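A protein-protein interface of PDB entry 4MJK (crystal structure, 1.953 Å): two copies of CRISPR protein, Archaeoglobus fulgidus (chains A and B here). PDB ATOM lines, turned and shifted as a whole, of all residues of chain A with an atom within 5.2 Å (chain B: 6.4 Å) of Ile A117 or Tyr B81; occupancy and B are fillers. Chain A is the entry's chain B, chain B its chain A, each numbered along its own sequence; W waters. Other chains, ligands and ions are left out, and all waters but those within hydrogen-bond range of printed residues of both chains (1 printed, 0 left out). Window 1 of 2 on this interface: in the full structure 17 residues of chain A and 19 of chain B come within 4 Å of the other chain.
Water W1 lies within hydrogen-bond range of NZ of Lys B115 and O of Val A11.
N of Thr A77 sits at hydrogen-bond distance from O of Ser A119 (2.9 Å). The backbone NH (N) of Leu B79 lies within hydrogen-bond range of the backbone carbonyl oxygen (O) of Ile B117 (2.7 Å). O of Trp A12 sits at hydrogen-bond distance from N of Leu A118, at 3.0 Å. O of Lys B115 lies within hydrogen-bond range of N of Tyr B81 (3.1 Å). The backbone NH (N) of Leu A79 sits at hydrogen-bond distance from the backbone carbonyl oxygen (O) of Ile A117. The backbone NH (N) of Tyr A81 sits at hydrogen-bond distance from the backbone carbonyl oxygen (O) of Lys A115.
OD1 of Asn B85 sits at hydrogen-bond distance from OG of Ser A119, 2.4 Å away. The side-chain hydroxyl (OH) of Tyr A81 lies within hydrogen-bond range of the side-chain hydroxyl (OG) of Ser B119 (2.6 Å). O of Trp A12 is in hydrogen-bond range of OH of Tyr B81. The backbone carbonyl oxygen of Val A11 sits at hydrogen-bond distance from the side-chain amino group of Lys B115. The backbone carbonyl oxygen (O) of Leu A118 is in hydrogen-bond range of the side-chain hydroxyl (OH) of Tyr B81, 3.1 Å away.
Val A11 touches Trp B12. Trp B12 touches Trp A12 (CB to CD1, 3.3 Å). Trp A12 touches Ile B117 (CB to CD1, 3.9 Å). OH of Tyr A81 touches CD2 of Leu B79, 3.9 Å away. Tyr A81 touches Ile B117. Leu B79 touches Ile A84. Ile A117 touches Tyr B81. Ile A117 touches Ile B84. Ile A117 touches Ile B117.
Trp A12 touches Ile B117, but with the chains exchanged Ile A117 does not touch Trp B12 (7.5 Å). Ile A84 touches Leu B79, but with the chains exchanged Leu A79 does not touch Ile B84 (4.03 Å). Ile A117 touches Ile B84, but with the chains exchanged Ile A84 does not touch Ile B117 (7.0 Å). Ile A117 touches its own counterpart, Ile B117.
Printed residues of chain B that touch a printed residue of chain A: Trp B12, Leu B79, Tyr B81, Ile B84, Asn B85, Lys B115, Ile B117 and Ser B119. Hydrophobic or aromatic side chains of chain B that line the printed part of chain A: Trp B12, Leu B79, Tyr B81, Ile B84 and Ile B117. Of the 14 printed residues of chain A, 7 touch a printed residue of chain B. Along chain A the printed residues that touch a printed residue of chain B span positions 11 to 119. Among the printed residues, 14 pairs touch across the chains. Among the printed residues, no Asp or Glu carboxylate lies within 4 Å of a Lys or Arg side-chain nitrogen of the other chain.
Ile A117 touches just these residues of chain B: Tyr B81 (3.6 Å), Ile B84 (3.96 Å) and Ile B117 (3.1 Å). Of chain A, only Trp A12 (3.2 Å), Ile A117 (3.6 Å) and Leu A118 (3.1 Å) come within 4 Å of Tyr B81. Of the printed residues of chain A, Leu B79 touches Tyr A81 and Ile A84. Of the printed residues of chain A, Ser B119 touches Tyr A81 (2.6 Å). Printed residues of chain B within 4 Å of Ser A119: Asn B85 (2.4 Å). Of the printed residues of chain B, Tyr A81 touches Leu B79 (3.9 Å), Ile B117 (3.5 Å) and Ser B119 (2.6 Å). Leu A79 touches none of the printed residues of chain B.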
ATOM      1  N   VAL A  11       6.168  13.760  -9.007  1.00  0.00           N
ATOM      2  CA  VAL A  11       6.777  14.687  -8.068  1.00  0.00           C
ATOM      3  C   VAL A  11       6.219  16.092  -8.219  1.00  0.00           C
ATOM      4  O   VAL A  11       5.859  16.732  -7.227  1.00  0.00           O
ATOM      5  CB  VAL A  11       8.315  14.710  -8.218  1.00  0.00           C
ATOM      6  CG1 VAL A  11       8.928  15.882  -7.416  1.00  0.00           C
ATOM      7  CG2 VAL A  11       8.911  13.356  -7.781  1.00  0.00           C
ATOM      8  N   TRP A  12       6.148  16.577  -9.457  1.00  0.00           N
ATOM      9  CA  TRP A  12       5.757  17.958  -9.702  1.00  0.00           C
ATOM     10  C   TRP A  12       4.924  18.154 -10.975  1.00  0.00           C
ATOM     11  O   TRP A  12       4.193  19.136 -11.086  1.00  0.00           O
ATOM     12  CB  TRP A  12       7.002  18.864  -9.776  1.00  0.00           C
ATOM     13  CG  TRP A  12       7.920  18.495 -10.916  1.00  0.00           C
ATOM     14  CD1 TRP A  12       8.957  17.616 -10.874  1.00  0.00           C
ATOM     15  CD2 TRP A  12       7.849  18.971 -12.274  1.00  0.00           C
ATOM     16  NE1 TRP A  12       9.548  17.517 -12.118  1.00  0.00           N
ATOM     17  CE2 TRP A  12       8.883  18.337 -12.993  1.00  0.00           C
ATOM     18  CE3 TRP A  12       7.010  19.872 -12.950  1.00  0.00           C
ATOM     19  CZ2 TRP A  12       9.113  18.582 -14.350  1.00  0.00           C
ATOM     20  CZ3 TRP A  12       7.240  20.114 -14.303  1.00  0.00           C
ATOM     21  CH2 TRP A  12       8.278  19.461 -14.990  1.00  0.00           C
ATOM     22  N   GLY A  13       5.060  17.245 -11.935  1.00  0.00           N
ATOM     23  CA  GLY A  13       4.501  17.456 -13.262  1.00  0.00           C
ATOM     24  C   GLY A  13       5.408  16.846 -14.311  1.00  0.00           C
ATOM     25  O   GLY A  13       6.146  15.900 -14.021  1.00  0.00           O
ATOM     26  N   THR A  77      -5.120  18.259 -10.779  1.00  0.00           N
ATOM     27  CA  THR A  77      -5.476  19.150 -11.866  1.00  0.00           C
ATOM     28  C   THR A  77      -4.185  19.712 -12.472  1.00  0.00           C
ATOM     29  O   THR A  77      -3.234  20.027 -11.751  1.00  0.00           O
ATOM     30  CB  THR A  77      -6.331  20.354 -11.353  1.00  0.00           C
ATOM     31  OG1 THR A  77      -7.294  19.898 -10.397  1.00  0.00           O
ATOM     32  CG2 THR A  77      -7.060  21.047 -12.518  1.00  0.00           C
ATOM     33  N   PRO A  78      -4.138  19.845 -13.801  1.00  0.00           N
ATOM     34  CA  PRO A  78      -2.897  20.377 -14.378  1.00  0.00           C
ATOM     35  C   PRO A  78      -2.906  21.890 -14.492  1.00  0.00           C
ATOM     36  O   PRO A  78      -3.971  22.487 -14.655  1.00  0.00           O
ATOM     37  CB  PRO A  78      -2.838  19.726 -15.777  1.00  0.00           C
ATOM     38  CG  PRO A  78      -4.269  19.417 -16.108  1.00  0.00           C
ATOM     39  CD  PRO A  78      -5.018  19.221 -14.806  1.00  0.00           C
ATOM     40  N   LEU A  79      -1.726  22.498 -14.391  1.00  0.00           N
ATOM     41  CA  LEU A  79      -1.560  23.908 -14.694  1.00  0.00           C
ATOM     42  C   LEU A  79      -0.410  24.065 -15.689  1.00  0.00           C
ATOM     43  O   LEU A  79       0.764  23.853 -15.344  1.00  0.00           O
ATOM     44  CB  LEU A  79      -1.254  24.696 -13.417  1.00  0.00           C
ATOM     45  CG  LEU A  79      -1.002  26.189 -13.608  1.00  0.00           C
ATOM     46  CD1 LEU A  79      -2.270  26.865 -14.149  1.00  0.00           C
ATOM     47  CD2 LEU A  79      -0.536  26.851 -12.305  1.00  0.00           C
ATOM     48  N   ARG A  80      -0.741  24.426 -16.922  1.00  0.00           N
ATOM     49  CA  ARG A  80       0.263  24.525 -17.975  1.00  0.00           C
ATOM     50  C   ARG A  80       1.145  25.751 -17.786  1.00  0.00           C
ATOM     51  O   ARG A  80       0.676  26.801 -17.361  1.00  0.00           O
ATOM     52  CB  ARG A  80      -0.422  24.549 -19.348  1.00  0.00           C
ATOM     53  CG  ARG A  80      -1.251  23.282 -19.630  1.00  0.00           C
ATOM     54  CD  ARG A  80      -2.174  23.501 -20.822  1.00  0.00           C
ATOM     55  NE  ARG A  80      -3.123  24.589 -20.579  1.00  0.00           N
ATOM     56  CZ  ARG A  80      -3.853  25.175 -21.522  1.00  0.00           C
ATOM     57  NH1 ARG A  80      -3.733  24.795 -22.791  1.00  0.00           N
ATOM     58  NH2 ARG A  80      -4.694  26.151 -21.195  1.00  0.00           N
ATOM     59  N   TYR A  81       2.429  25.622 -18.098  1.00  0.00           N
ATOM     60  CA  TYR A  81       3.335  26.757 -17.949  1.00  0.00           C
ATOM     61  C   TYR A  81       2.957  27.928 -18.843  1.00  0.00           C
ATOM     62  O   TYR A  81       3.322  29.072 -18.559  1.00  0.00           O
ATOM     63  CB  TYR A  81       4.782  26.350 -18.201  1.00  0.00           C
ATOM     64  CG  TYR A  81       5.568  26.152 -16.925  1.00  0.00           C
ATOM     65  CD1 TYR A  81       5.545  24.937 -16.254  1.00  0.00           C
ATOM     66  CD2 TYR A  81       6.339  27.186 -16.389  1.00  0.00           C
ATOM     67  CE1 TYR A  81       6.275  24.753 -15.084  1.00  0.00           C
ATOM     68  CE2 TYR A  81       7.064  27.005 -15.226  1.00  0.00           C
ATOM     69  CZ  TYR A  81       7.032  25.787 -14.582  1.00  0.00           C
ATOM     70  OH  TYR A  81       7.752  25.602 -13.425  1.00  0.00           O
ATOM     71  N   ILE A  84       0.831  29.965 -16.436  1.00  0.00           N
ATOM     72  CA  ILE A  84       1.666  30.566 -15.403  1.00  0.00           C
ATOM     73  C   ILE A  84       2.473  31.730 -15.960  1.00  0.00           C
ATOM     74  O   ILE A  84       2.572  32.795 -15.329  1.00  0.00           O
ATOM     75  CB  ILE A  84       2.657  29.534 -14.845  1.00  0.00           C
ATOM     76  CG1 ILE A  84       1.904  28.426 -14.100  1.00  0.00           C
ATOM     77  CG2 ILE A  84       3.688  30.227 -13.936  1.00  0.00           C
ATOM     78  CD1 ILE A  84       2.708  27.141 -13.919  1.00  0.00           C
ATOM     79  N   LYS A 115       5.617  21.959 -20.958  1.00  0.00           N
ATOM     80  CA  LYS A 115       5.814  21.763 -19.519  1.00  0.00           C
ATOM     81  C   LYS A 115       4.594  22.149 -18.706  1.00  0.00           C
ATOM     82  O   LYS A 115       4.001  23.212 -18.922  1.00  0.00           O
ATOM     83  CB  LYS A 115       7.027  22.536 -18.997  1.00  0.00           C
ATOM     84  CG  LYS A 115       7.254  22.315 -17.504  1.00  0.00           C
ATOM     85  CD  LYS A 115       8.714  22.557 -17.076  1.00  0.00           C
ATOM     86  CE  LYS A 115       9.125  24.003 -17.254  1.00  0.00           C
ATOM     87  NZ  LYS A 115      10.474  24.304 -16.627  1.00  0.00           N
ATOM     88  N   THR A 116       4.241  21.292 -17.748  1.00  0.00           N
ATOM     89  CA  THR A 116       2.968  21.412 -17.043  1.00  0.00           C
ATOM     90  C   THR A 116       3.110  20.952 -15.609  1.00  0.00           C
ATOM     91  O   THR A 116       3.755  19.949 -15.339  1.00  0.00           O
ATOM     92  CB  THR A 116       1.908  20.562 -17.755  1.00  0.00           C
ATOM     93  OG1 THR A 116       1.727  21.073 -19.082  1.00  0.00           O
ATOM     94  CG2 THR A 116       0.571  20.575 -17.013  1.00  0.00           C
ATOM     95  N   ILE A 117       2.521  21.698 -14.685  1.00  0.00           N
ATOM     96  CA  ILE A 117       2.568  21.328 -13.279  1.00  0.00           C
ATOM     97  C   ILE A 117       1.311  20.541 -12.947  1.00  0.00           C
ATOM     98  O   ILE A 117       0.254  20.823 -13.497  1.00  0.00           O
ATOM     99  CB  ILE A 117       2.588  22.587 -12.397  1.00  0.00           C
ATOM    100  CG1 ILE A 117       3.769  23.474 -12.779  1.00  0.00           C
ATOM    101  CG2 ILE A 117       2.596  22.224 -10.927  1.00  0.00           C
ATOM    102  CD1 ILE A 117       5.084  22.809 -12.678  1.00  0.00           C
ATOM    103  N   LEU A 118       1.426  19.548 -12.067  1.00  0.00           N
ATOM    104  CA  LEU A 118       0.248  18.854 -11.554  1.00  0.00           C
ATOM    105  C   LEU A 118       0.059  19.217 -10.081  1.00  0.00           C
ATOM    106  O   LEU A 118       1.018  19.194  -9.287  1.00  0.00           O
ATOM    107  CB  LEU A 118       0.386  17.329 -11.724  1.00  0.00           C
ATOM    108  CG  LEU A 118       0.433  16.811 -13.172  1.00  0.00           C
ATOM    109  CD1 LEU A 118       0.928  15.364 -13.227  1.00  0.00           C
ATOM    110  CD2 LEU A 118      -0.932  16.963 -13.873  1.00  0.00           C
ATOM    111  N   SER A 119      -1.165  19.570  -9.710  1.00  0.00           N
ATOM    112  CA  SER A 119      -1.439  19.915  -8.323  1.00  0.00           C
ATOM    113  C   SER A 119      -2.573  19.067  -7.770  1.00  0.00           C
ATOM    114  O   SER A 119      -3.611  18.938  -8.398  1.00  0.00           O
ATOM    115  CB  SER A 119      -1.794  21.399  -8.202  1.00  0.00           C
ATOM    116  OG  SER A 119      -2.096  21.708  -6.850  1.00  0.00           O
ATOM    117  N   TRP B  12      14.314  19.392  -9.959  1.00  0.00           N
ATOM    118  CA  TRP B  12      12.990  20.036 -10.136  1.00  0.00           C
ATOM    119  C   TRP B  12      12.668  21.155  -9.144  1.00  0.00           C
ATOM    120  O   TRP B  12      11.805  21.988  -9.416  1.00  0.00           O
ATOM    121  CB  TRP B  12      11.865  18.990 -10.017  1.00  0.00           C
ATOM    122  CG  TRP B  12      11.813  18.358  -8.651  1.00  0.00           C
ATOM    123  CD1 TRP B  12      12.478  17.232  -8.235  1.00  0.00           C
ATOM    124  CD2 TRP B  12      11.098  18.843  -7.507  1.00  0.00           C
ATOM    125  NE1 TRP B  12      12.195  16.981  -6.912  1.00  0.00           N
ATOM    126  CE2 TRP B  12      11.354  17.956  -6.444  1.00  0.00           C
ATOM    127  CE3 TRP B  12      10.248  19.932  -7.285  1.00  0.00           C
ATOM    128  CZ2 TRP B  12      10.801  18.135  -5.164  1.00  0.00           C
ATOM    129  CZ3 TRP B  12       9.700  20.105  -6.017  1.00  0.00           C
ATOM    130  CH2 TRP B  12       9.981  19.211  -4.977  1.00  0.00           C
ATOM    131  N   SER B  27       5.729  29.342   3.601  1.00  0.00           N
ATOM    132  CA  SER B  27       6.224  28.731   2.365  1.00  0.00           C
ATOM    133  C   SER B  27       7.585  29.364   2.051  1.00  0.00           C
ATOM    134  O   SER B  27       7.953  30.386   2.646  1.00  0.00           O
ATOM    135  CB  SER B  27       5.250  28.961   1.221  1.00  0.00           C
ATOM    136  OG  SER B  27       5.056  30.348   1.012  1.00  0.00           O
ATOM    137  N   LEU B  79       8.862  28.798  -7.906  1.00  0.00           N
ATOM    138  CA  LEU B  79       7.417  28.852  -8.061  1.00  0.00           C
ATOM    139  C   LEU B  79       6.853  28.036  -6.911  1.00  0.00           C
ATOM    140  O   LEU B  79       6.895  26.815  -6.942  1.00  0.00           O
ATOM    141  CB  LEU B  79       7.006  28.264  -9.424  1.00  0.00           C
ATOM    142  CG  LEU B  79       5.510  28.208  -9.726  1.00  0.00           C
ATOM    143  CD1 LEU B  79       4.931  29.610  -9.844  1.00  0.00           C
ATOM    144  CD2 LEU B  79       5.235  27.395 -11.012  1.00  0.00           C
ATOM    145  N   ARG B  80       6.382  28.714  -5.871  1.00  0.00           N
ATOM    146  CA  ARG B  80       5.925  28.021  -4.675  1.00  0.00           C
ATOM    147  C   ARG B  80       4.604  27.332  -4.983  1.00  0.00           C
ATOM    148  O   ARG B  80       3.824  27.820  -5.801  1.00  0.00           O
ATOM    149  CB  ARG B  80       5.753  29.007  -3.524  1.00  0.00           C
ATOM    150  CG  ARG B  80       7.024  29.757  -3.176  1.00  0.00           C
ATOM    151  CD  ARG B  80       6.715  30.899  -2.229  1.00  0.00           C
ATOM    152  NE  ARG B  80       5.809  31.861  -2.844  1.00  0.00           N
ATOM    153  CZ  ARG B  80       5.127  32.780  -2.169  1.00  0.00           C
ATOM    154  NH1 ARG B  80       5.247  32.860  -0.844  1.00  0.00           N
ATOM    155  NH2 ARG B  80       4.315  33.611  -2.812  1.00  0.00           N
ATOM    156  N   TYR B  81       4.339  26.201  -4.341  1.00  0.00           N
ATOM    157  CA  TYR B  81       3.049  25.567  -4.592  1.00  0.00           C
ATOM    158  C   TYR B  81       1.922  26.461  -4.089  1.00  0.00           C
ATOM    159  O   TYR B  81       0.793  26.394  -4.573  1.00  0.00           O
ATOM    160  CB  TYR B  81       2.975  24.150  -4.024  1.00  0.00           C
ATOM    161  CG  TYR B  81       3.150  23.110  -5.108  1.00  0.00           C
ATOM    162  CD1 TYR B  81       4.397  22.570  -5.380  1.00  0.00           C
ATOM    163  CD2 TYR B  81       2.069  22.697  -5.889  1.00  0.00           C
ATOM    164  CE1 TYR B  81       4.566  21.633  -6.384  1.00  0.00           C
ATOM    165  CE2 TYR B  81       2.226  21.754  -6.904  1.00  0.00           C
ATOM    166  CZ  TYR B  81       3.481  21.233  -7.143  1.00  0.00           C
ATOM    167  OH  TYR B  81       3.669  20.292  -8.128  1.00  0.00           O
ATOM    168  N   SER B  82       2.235  27.336  -3.141  1.00  0.00           N
ATOM    169  CA  SER B  82       1.229  28.305  -2.720  1.00  0.00           C
ATOM    170  C   SER B  82       0.875  29.254  -3.873  1.00  0.00           C
ATOM    171  O   SER B  82      -0.290  29.623  -4.017  1.00  0.00           O
ATOM    172  CB  SER B  82       1.637  29.052  -1.435  1.00  0.00           C
ATOM    173  OG  SER B  82       2.606  30.047  -1.684  1.00  0.00           O
ATOM    174  N   ASP B  83       1.864  29.618  -4.701  1.00  0.00           N
ATOM    175  CA  ASP B  83       1.629  30.421  -5.920  1.00  0.00           C
ATOM    176  C   ASP B  83       0.786  29.626  -6.929  1.00  0.00           C
ATOM    177  O   ASP B  83      -0.164  30.136  -7.533  1.00  0.00           O
ATOM    178  CB  ASP B  83       2.955  30.772  -6.607  1.00  0.00           C
ATOM    179  CG  ASP B  83       3.804  31.757  -5.812  1.00  0.00           C
ATOM    180  OD1 ASP B  83       3.231  32.733  -5.282  1.00  0.00           O
ATOM    181  OD2 ASP B  83       5.045  31.553  -5.729  1.00  0.00           O
ATOM    182  N   ILE B  84       1.170  28.369  -7.118  1.00  0.00           N
ATOM    183  CA  ILE B  84       0.495  27.484  -8.048  1.00  0.00           C
ATOM    184  C   ILE B  84      -0.976  27.262  -7.680  1.00  0.00           C
ATOM    185  O   ILE B  84      -1.862  27.366  -8.537  1.00  0.00           O
ATOM    186  CB  ILE B  84       1.210  26.127  -8.116  1.00  0.00           C
ATOM    187  CG1 ILE B  84       2.529  26.262  -8.887  1.00  0.00           C
ATOM    188  CG2 ILE B  84       0.293  25.072  -8.761  1.00  0.00           C
ATOM    189  CD1 ILE B  84       3.581  25.198  -8.504  1.00  0.00           C
ATOM    190  N   ASN B  85      -1.232  26.941  -6.414  1.00  0.00           N
ATOM    191  CA  ASN B  85      -2.591  26.636  -5.982  1.00  0.00           C
ATOM    192  C   ASN B  85      -3.452  27.896  -6.015  1.00  0.00           C
ATOM    193  O   ASN B  85      -4.660  27.821  -6.213  1.00  0.00           O
ATOM    194  CB  ASN B  85      -2.600  25.929  -4.619  1.00  0.00           C
ATOM    195  CG  ASN B  85      -2.062  24.508  -4.713  1.00  0.00           C
ATOM    196  OD1 ASN B  85      -2.056  23.917  -5.793  1.00  0.00           O
ATOM    197  ND2 ASN B  85      -1.599  23.956  -3.596  1.00  0.00           N
ATOM    198  N   ARG B  86      -2.803  29.050  -5.868  1.00  0.00           N
ATOM    199  CA  ARG B  86      -3.459  30.344  -6.052  1.00  0.00           C
ATOM    200  C   ARG B  86      -3.861  30.594  -7.513  1.00  0.00           C
ATOM    201  O   ARG B  86      -5.016  30.926  -7.796  1.00  0.00           O
ATOM    202  CB  ARG B  86      -2.548  31.471  -5.573  1.00  0.00           C
ATOM    203  CG  ARG B  86      -3.268  32.532  -4.749  1.00  0.00           C
ATOM    204  CD  ARG B  86      -2.320  33.630  -4.276  1.00  0.00           C
ATOM    205  NE  ARG B  86      -3.041  34.788  -3.745  1.00  0.00           N
ATOM    206  CZ  ARG B  86      -2.452  35.879  -3.260  1.00  0.00           C
ATOM    207  NH1 ARG B  86      -1.126  35.966  -3.230  1.00  0.00           N
ATOM    208  NH2 ARG B  86      -3.187  36.884  -2.803  1.00  0.00           N
ATOM    209  N   ALA B 112       2.132  19.243   1.454  1.00  0.00           N
ATOM    210  CA  ALA B 112       3.002  19.886   0.472  1.00  0.00           C
ATOM    211  C   ALA B 112       3.563  21.200   1.021  1.00  0.00           C
ATOM    212  O   ALA B 112       3.883  22.120   0.258  1.00  0.00           O
ATOM    213  CB  ALA B 112       2.232  20.139  -0.832  1.00  0.00           C
ATOM    214  N   LYS B 115       6.953  23.156  -0.246  1.00  0.00           N
ATOM    215  CA  LYS B 115       7.320  22.560  -1.528  1.00  0.00           C
ATOM    216  C   LYS B 115       7.297  23.597  -2.636  1.00  0.00           C
ATOM    217  O   LYS B 115       6.308  24.311  -2.811  1.00  0.00           O
ATOM    218  CB  LYS B 115       6.416  21.387  -1.876  1.00  0.00           C
ATOM    219  CG  LYS B 115       6.813  20.656  -3.162  1.00  0.00           C
ATOM    220  CD  LYS B 115       5.925  19.438  -3.376  1.00  0.00           C
ATOM    221  CE  LYS B 115       6.433  18.563  -4.519  1.00  0.00           C
ATOM    222  NZ  LYS B 115       5.632  17.284  -4.636  1.00  0.00           N
ATOM    223  N   THR B 116       8.394  23.655  -3.388  1.00  0.00           N
ATOM    224  CA  THR B 116       8.637  24.738  -4.332  1.00  0.00           C
ATOM    225  C   THR B 116       9.308  24.229  -5.587  1.00  0.00           C
ATOM    226  O   THR B 116      10.289  23.483  -5.515  1.00  0.00           O
ATOM    227  CB  THR B 116       9.530  25.813  -3.671  1.00  0.00           C
ATOM    228  OG1 THR B 116       8.810  26.391  -2.582  1.00  0.00           O
ATOM    229  CG2 THR B 116       9.914  26.916  -4.653  1.00  0.00           C
ATOM    230  N   ILE B 117       8.772  24.614  -6.744  1.00  0.00           N
ATOM    231  CA  ILE B 117       9.386  24.238  -8.013  1.00  0.00           C
ATOM    232  C   ILE B 117      10.424  25.304  -8.391  1.00  0.00           C
ATOM    233  O   ILE B 117      10.217  26.486  -8.154  1.00  0.00           O
ATOM    234  CB  ILE B 117       8.292  24.089  -9.122  1.00  0.00           C
ATOM    235  CG1 ILE B 117       7.446  22.838  -8.851  1.00  0.00           C
ATOM    236  CG2 ILE B 117       8.911  24.041 -10.523  1.00  0.00           C
ATOM    237  CD1 ILE B 117       6.236  22.727  -9.749  1.00  0.00           C
ATOM    238  N   SER B 119      11.906  26.925 -11.533  1.00  0.00           N
ATOM    239  CA  SER B 119      11.692  26.994 -12.978  1.00  0.00           C
ATOM    240  C   SER B 119      12.913  27.605 -13.662  1.00  0.00           C
ATOM    241  O   SER B 119      13.263  28.757 -13.421  1.00  0.00           O
ATOM    242  CB  SER B 119      10.477  27.869 -13.309  1.00  0.00           C
ATOM    243  OG  SER B 119       9.340  27.507 -12.552  1.00  0.00           O
HETATM  244  O   HOH W   1       4.781  14.560  -5.059  1.00  0.00           O
